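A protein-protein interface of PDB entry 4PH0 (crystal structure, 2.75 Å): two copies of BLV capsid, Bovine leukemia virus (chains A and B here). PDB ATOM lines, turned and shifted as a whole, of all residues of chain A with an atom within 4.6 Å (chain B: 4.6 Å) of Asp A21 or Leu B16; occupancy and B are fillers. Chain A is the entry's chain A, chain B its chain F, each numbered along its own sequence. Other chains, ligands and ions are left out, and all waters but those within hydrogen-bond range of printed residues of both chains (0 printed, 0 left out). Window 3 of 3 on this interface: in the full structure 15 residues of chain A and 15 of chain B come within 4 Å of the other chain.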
ATOM      1  N   ARG A  17      20.915 -21.550  15.766  1.00  0.00           N
ATOM      2  CA  ARG A  17      20.281 -21.961  17.020  1.00  0.00           C
ATOM      3  C   ARG A  17      20.995 -23.158  17.630  1.00  0.00           C
ATOM      4  O   ARG A  17      21.189 -23.207  18.843  1.00  0.00           O
ATOM      5  CB  ARG A  17      18.791 -22.263  16.862  1.00  0.00           C
ATOM      6  CG  ARG A  17      18.135 -22.493  18.227  1.00  0.00           C
ATOM      7  CD  ARG A  17      18.259 -21.221  19.088  1.00  0.00           C
ATOM      8  NE  ARG A  17      17.706 -21.374  20.434  1.00  0.00           N
ATOM      9  CZ  ARG A  17      17.999 -20.586  21.468  1.00  0.00           C
ATOM     10  NH1 ARG A  17      18.859 -19.587  21.327  1.00  0.00           N
ATOM     11  NH2 ARG A  17      17.443 -20.812  22.651  1.00  0.00           N
ATOM     12  N   GLU A  18      21.379 -24.123  16.800  1.00  0.00           N
ATOM     13  CA  GLU A  18      22.113 -25.282  17.301  1.00  0.00           C
ATOM     14  C   GLU A  18      23.293 -24.833  18.131  1.00  0.00           C
ATOM     15  O   GLU A  18      23.512 -25.325  19.233  1.00  0.00           O
ATOM     16  CB  GLU A  18      22.620 -26.152  16.165  1.00  0.00           C
ATOM     17  CG  GLU A  18      21.541 -26.852  15.419  1.00  0.00           C
ATOM     18  CD  GLU A  18      22.069 -27.594  14.219  1.00  0.00           C
ATOM     19  OE1 GLU A  18      22.996 -27.082  13.554  1.00  0.00           O
ATOM     20  OE2 GLU A  18      21.550 -28.691  13.933  1.00  0.00           O
ATOM     21  N   LEU A  19      24.034 -23.876  17.585  1.00  0.00           N
ATOM     22  CA  LEU A  19      25.228 -23.306  18.202  1.00  0.00           C
ATOM     23  C   LEU A  19      24.890 -22.535  19.463  1.00  0.00           C
ATOM     24  O   LEU A  19      25.589 -22.628  20.474  1.00  0.00           O
ATOM     25  CB  LEU A  19      25.886 -22.359  17.208  1.00  0.00           C
ATOM     26  CG  LEU A  19      26.194 -23.015  15.867  1.00  0.00           C
ATOM     27  CD1 LEU A  19      26.266 -21.967  14.789  1.00  0.00           C
ATOM     28  CD2 LEU A  19      27.492 -23.789  15.944  1.00  0.00           C
ATOM     29  N   GLN A  20      23.814 -21.758  19.366  1.00  0.00           N
ATOM     30  CA  GLN A  20      23.354 -20.916  20.454  1.00  0.00           C
ATOM     31  C   GLN A  20      22.935 -21.771  21.624  1.00  0.00           C
ATOM     32  O   GLN A  20      23.203 -21.429  22.773  1.00  0.00           O
ATOM     33  CB  GLN A  20      22.189 -20.031  20.024  1.00  0.00           C
ATOM     34  CG  GLN A  20      22.546 -18.977  19.020  1.00  0.00           C
ATOM     35  CD  GLN A  20      21.362 -18.154  18.599  1.00  0.00           C
ATOM     36  OE1 GLN A  20      20.283 -18.683  18.348  1.00  0.00           O
ATOM     37  NE2 GLN A  20      21.558 -16.844  18.510  1.00  0.00           N
ATOM     38  N   ASP A  21      22.281 -22.888  21.317  1.00  0.00           N
ATOM     39  CA  ASP A  21      21.778 -23.773  22.354  1.00  0.00           C
ATOM     40  C   ASP A  21      22.916 -24.240  23.223  1.00  0.00           C
ATOM     41  O   ASP A  21      22.866 -24.160  24.450  1.00  0.00           O
ATOM     42  CB  ASP A  21      21.098 -25.008  21.753  1.00  0.00           C
ATOM     43  CG  ASP A  21      19.762 -24.713  21.127  1.00  0.00           C
ATOM     44  OD1 ASP A  21      19.209 -23.622  21.366  1.00  0.00           O
ATOM     45  OD2 ASP A  21      19.257 -25.603  20.408  1.00  0.00           O
ATOM     46  N   ILE A  22      23.952 -24.724  22.560  1.00  0.00           N
ATOM     47  CA  ILE A  22      25.104 -25.243  23.252  1.00  0.00           C
ATOM     48  C   ILE A  22      25.741 -24.139  24.069  1.00  0.00           C
ATOM     49  O   ILE A  22      26.030 -24.339  25.243  1.00  0.00           O
ATOM     50  CB  ILE A  22      26.109 -25.837  22.284  1.00  0.00           C
ATOM     51  CG1 ILE A  22      25.472 -26.996  21.523  1.00  0.00           C
ATOM     52  CG2 ILE A  22      27.310 -26.323  23.031  1.00  0.00           C
ATOM     53  CD1 ILE A  22      26.282 -27.502  20.380  1.00  0.00           C
ATOM     54  N   LYS A  23      25.933 -22.972  23.458  1.00  0.00           N
ATOM     55  CA  LYS A  23      26.484 -21.826  24.173  1.00  0.00           C
ATOM     56  C   LYS A  23      25.663 -21.605  25.430  1.00  0.00           C
ATOM     57  O   LYS A  23      26.208 -21.507  26.528  1.00  0.00           O
ATOM     58  CB  LYS A  23      26.498 -20.572  23.309  1.00  0.00           C
ATOM     59  CG  LYS A  23      27.164 -19.383  23.991  1.00  0.00           C
ATOM     60  CD  LYS A  23      27.104 -18.136  23.123  1.00  0.00           C
ATOM     61  CE  LYS A  23      28.064 -17.055  23.598  1.00  0.00           C
ATOM     62  NZ  LYS A  23      27.605 -16.403  24.847  1.00  0.00           N
ATOM     63  N   LYS A  24      24.348 -21.524  25.258  1.00  0.00           N
ATOM     64  CA  LYS A  24      23.453 -21.328  26.383  1.00  0.00           C
ATOM     65  C   LYS A  24      23.683 -22.417  27.400  1.00  0.00           C
ATOM     66  O   LYS A  24      23.733 -22.171  28.596  1.00  0.00           O
ATOM     67  CB  LYS A  24      22.000 -21.352  25.937  1.00  0.00           C
ATOM     68  CG  LYS A  24      21.009 -21.226  27.083  1.00  0.00           C
ATOM     69  CD  LYS A  24      19.596 -21.408  26.575  1.00  0.00           C
ATOM     70  CE  LYS A  24      19.255 -22.870  26.484  1.00  0.00           C
ATOM     71  NZ  LYS A  24      17.912 -23.095  25.908  1.00  0.00           N
ATOM     72  N   GLU A  25      23.824 -23.635  26.912  1.00  0.00           N
ATOM     73  CA  GLU A  25      23.998 -24.752  27.807  1.00  0.00           C
ATOM     74  C   GLU A  25      25.305 -24.650  28.570  1.00  0.00           C
ATOM     75  O   GLU A  25      25.344 -24.817  29.780  1.00  0.00           O
ATOM     76  CB  GLU A  25      23.944 -26.065  27.037  1.00  0.00           C
ATOM     77  CG  GLU A  25      23.986 -27.261  27.946  1.00  0.00           C
ATOM     78  CD  GLU A  25      22.889 -27.214  28.983  1.00  0.00           C
ATOM     79  OE1 GLU A  25      21.724 -26.975  28.604  1.00  0.00           O
ATOM     80  OE2 GLU A  25      23.190 -27.400  30.181  1.00  0.00           O
ATOM     81  N   GLN A  46      25.498 -35.499  18.072  1.00  0.00           N
ATOM     82  CA  GLN A  46      24.408 -34.927  17.302  1.00  0.00           C
ATOM     83  C   GLN A  46      24.724 -34.755  15.846  1.00  0.00           C
ATOM     84  O   GLN A  46      23.988 -35.190  14.962  1.00  0.00           O
ATOM     85  CB  GLN A  46      24.062 -33.516  17.778  1.00  0.00           C
ATOM     86  CG  GLN A  46      23.414 -33.344  19.117  1.00  0.00           C
ATOM     87  CD  GLN A  46      22.815 -31.930  19.246  1.00  0.00           C
ATOM     88  OE1 GLN A  46      23.494 -30.982  19.589  1.00  0.00           O
ATOM     89  NE2 GLN A  46      21.533 -31.796  18.904  1.00  0.00           N
ATOM     90  N   TRP B  14      21.062 -38.032  20.873  1.00  0.00           N
ATOM     91  CA  TRP B  14      20.201 -36.996  21.444  1.00  0.00           C
ATOM     92  C   TRP B  14      19.983 -35.677  20.727  1.00  0.00           C
ATOM     93  O   TRP B  14      20.807 -35.249  19.948  1.00  0.00           O
ATOM     94  CB  TRP B  14      20.699 -36.702  22.847  1.00  0.00           C
ATOM     95  CG  TRP B  14      20.059 -37.617  23.787  1.00  0.00           C
ATOM     96  CD1 TRP B  14      20.621 -38.634  24.494  1.00  0.00           C
ATOM     97  CD2 TRP B  14      18.673 -37.615  24.107  1.00  0.00           C
ATOM     98  NE1 TRP B  14      19.660 -39.259  25.259  1.00  0.00           N
ATOM     99  CE2 TRP B  14      18.453 -38.648  25.031  1.00  0.00           C
ATOM    100  CE3 TRP B  14      17.591 -36.828  23.704  1.00  0.00           C
ATOM    101  CZ2 TRP B  14      17.191 -38.913  25.558  1.00  0.00           C
ATOM    102  CZ3 TRP B  14      16.341 -37.093  24.222  1.00  0.00           C
ATOM    103  CH2 TRP B  14      16.149 -38.122  25.140  1.00  0.00           C
ATOM    104  N   ALA B  15      18.832 -35.055  20.964  1.00  0.00           N
ATOM    105  CA  ALA B  15      18.754 -33.634  20.669  1.00  0.00           C
ATOM    106  C   ALA B  15      19.003 -32.809  21.911  1.00  0.00           C
ATOM    107  O   ALA B  15      18.389 -33.012  22.945  1.00  0.00           O
ATOM    108  CB  ALA B  15      17.443 -33.288  20.069  1.00  0.00           C
ATOM    109  N   LEU B  16      19.908 -31.859  21.759  1.00  0.00           N
ATOM    110  CA  LEU B  16      20.230 -30.930  22.810  1.00  0.00           C
ATOM    111  C   LEU B  16      19.008 -30.160  23.296  1.00  0.00           C
ATOM    112  O   LEU B  16      18.793 -29.992  24.489  1.00  0.00           O
ATOM    113  CB  LEU B  16      21.267 -29.947  22.328  1.00  0.00           C
ATOM    114  CG  LEU B  16      21.603 -28.931  23.402  1.00  0.00           C
ATOM    115  CD1 LEU B  16      22.225 -29.679  24.545  1.00  0.00           C
ATOM    116  CD2 LEU B  16      22.504 -27.937  22.816  1.00  0.00           C
ATOM    117  N   ARG B  17      18.226 -29.653  22.351  1.00  0.00           N
ATOM    118  CA  ARG B  17      17.016 -28.900  22.679  1.00  0.00           C
ATOM    119  C   ARG B  17      16.119 -29.751  23.536  1.00  0.00           C
ATOM    120  O   ARG B  17      15.536 -29.268  24.504  1.00  0.00           O
ATOM    121  CB  ARG B  17      16.278 -28.412  21.421  1.00  0.00           C
ATOM    122  CG  ARG B  17      15.091 -27.471  21.686  1.00  0.00           C
ATOM    123  CD  ARG B  17      14.650 -26.788  20.396  1.00  0.00           C
ATOM    124  NE  ARG B  17      14.089 -27.708  19.408  1.00  0.00           N
ATOM    125  CZ  ARG B  17      12.809 -28.059  19.352  1.00  0.00           C
ATOM    126  NH1 ARG B  17      11.941 -27.552  20.222  1.00  0.00           N
ATOM    127  NH2 ARG B  17      12.400 -28.911  18.423  1.00  0.00           N
ATOM    128  N   GLU B  18      15.996 -31.021  23.157  1.00  0.00           N
ATOM    129  CA  GLU B  18      15.232 -31.977  23.948  1.00  0.00           C
ATOM    130  C   GLU B  18      15.753 -31.902  25.370  1.00  0.00           C
ATOM    131  O   GLU B  18      14.996 -31.753  26.321  1.00  0.00           O
ATOM    132  CB  GLU B  18      15.349 -33.401  23.394  1.00  0.00           C
ATOM    133  CG  GLU B  18      14.660 -33.608  22.048  1.00  0.00           C
ATOM    134  CD  GLU B  18      14.888 -34.997  21.471  1.00  0.00           C
ATOM    135  OE1 GLU B  18      15.993 -35.544  21.656  1.00  0.00           O
ATOM    136  OE2 GLU B  18      13.976 -35.526  20.799  1.00  0.00           O
ATOM    137  N   LEU B  19      17.069 -31.939  25.490  1.00  0.00           N
ATOM    138  CA  LEU B  19      17.724 -31.850  26.778  1.00  0.00           C
ATOM    139  C   LEU B  19      17.499 -30.465  27.389  1.00  0.00           C
ATOM    140  O   LEU B  19      17.373 -30.333  28.601  1.00  0.00           O
ATOM    141  CB  LEU B  19      19.207 -32.140  26.619  1.00  0.00           C
ATOM    142  CG  LEU B  19      19.547 -33.493  25.990  1.00  0.00           C
ATOM    143  CD1 LEU B  19      20.893 -33.404  25.350  1.00  0.00           C
ATOM    144  CD2 LEU B  19      19.580 -34.584  27.032  1.00  0.00           C
ATOM    145  N   GLN B  20      17.506 -29.432  26.547  1.00  0.00           N
ATOM    146  CA  GLN B  20      17.347 -28.058  27.010  1.00  0.00           C
ATOM    147  C   GLN B  20      16.000 -27.836  27.676  1.00  0.00           C
ATOM    148  O   GLN B  20      15.911 -27.206  28.728  1.00  0.00           O
ATOM    149  CB  GLN B  20      17.458 -27.084  25.836  1.00  0.00           C
ATOM    150  CG  GLN B  20      18.811 -26.986  25.163  1.00  0.00           C
ATOM    151  CD  GLN B  20      19.946 -26.810  26.133  1.00  0.00           C
ATOM    152  OE1 GLN B  20      20.281 -25.694  26.521  1.00  0.00           O
ATOM    153  NE2 GLN B  20      20.558 -27.914  26.524  1.00  0.00           N
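CD2 of Leu B16 touches CB of Asp A21 (3.4 Å). Gln B20 touches Asp A21. CD2 of Leu B16 touches CG1 of Ile A22, 3.4 Å away. Lys A24 touches Gln B20 (CE to OE1, 3.0 Å). CG of Gln A46 touches O of Trp B14 (3.3 Å). Ala B15 touches Gln A46 (CA to NE2, 3.8 Å).
Asp A21 touches just these residues of chain B: Leu B16 and Gln B20. Of the printed residues of chain B, Ile A22 touches Leu B16 (3.4 Å). Printed residues of chain B within 4 Å of Lys A24: Gln B20 (3.0 Å). Of the printed residues of chain B, Gln A46 touches Trp B14, Ala B15 and Leu B16. Printed residues of chain A within 4 Å of Trp B14: Gln A46 (3.3 Å). Leu B16 touches three residues of chain A. Leu B19 touches none of the printed residues of chain A. Of the printed residues of chain A, Gln B20 touches Asp A21, Lys A24 and Glu A25. The nearest residue of chain B that does not touch Asp A21 is Arg B17 (4.2 Å).
Positions printed for both chains: 17, 18, 19 and 20. Of the 8 pairs that touch across the chains among the printed residues, none has its exchanged pair printed and touching as well.
Printed residues of chain A that touch a printed residue of chain B: Asp A21, Ile A22, Lys A24, Glu A25 and Gln A46. Hydrophobic or aromatic side chains of chain A within 4 Å of the printed part of chain B: Ile A22. Of the 7 printed residues of chain B, 4 touch a printed residue of chain A. Printed residues of chain B that touch a printed residue of chain A: Trp B14, Ala B15, Leu B16 and Gln B20. Hydrophobic or aromatic side chains of chain B within 4 Å of the printed part of chain A: Leu B16. Among the printed residues, no Asp or Glu carboxylate lies within 4 Å of a Lys or Arg side-chain nitrogen of the other chain.
The side-chain carboxylate of Glu A25 lies within hydrogen-bond range of the side-chain amide nitrogen of Gln B20, 2.6 Å away. The side-chain amide nitrogen (NE2) of Gln A46 lies close to the backbone NH (N) of Leu B16 (3.3 Å).
The side-chain carboxylate of Asp A21 lies within salt-bridge range of the guanidinium group of Arg A17 (2.9 Å). The backbone NH (N) of Ala B15 sits at hydrogen-bond distance from the side-chain carboxylate (OE1) of Glu B18 (3.0 Å). The backbone carbonyl oxygen of Leu B16 sits close to the side-chain amide nitrogen of Gln B20 (3.4 Å).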
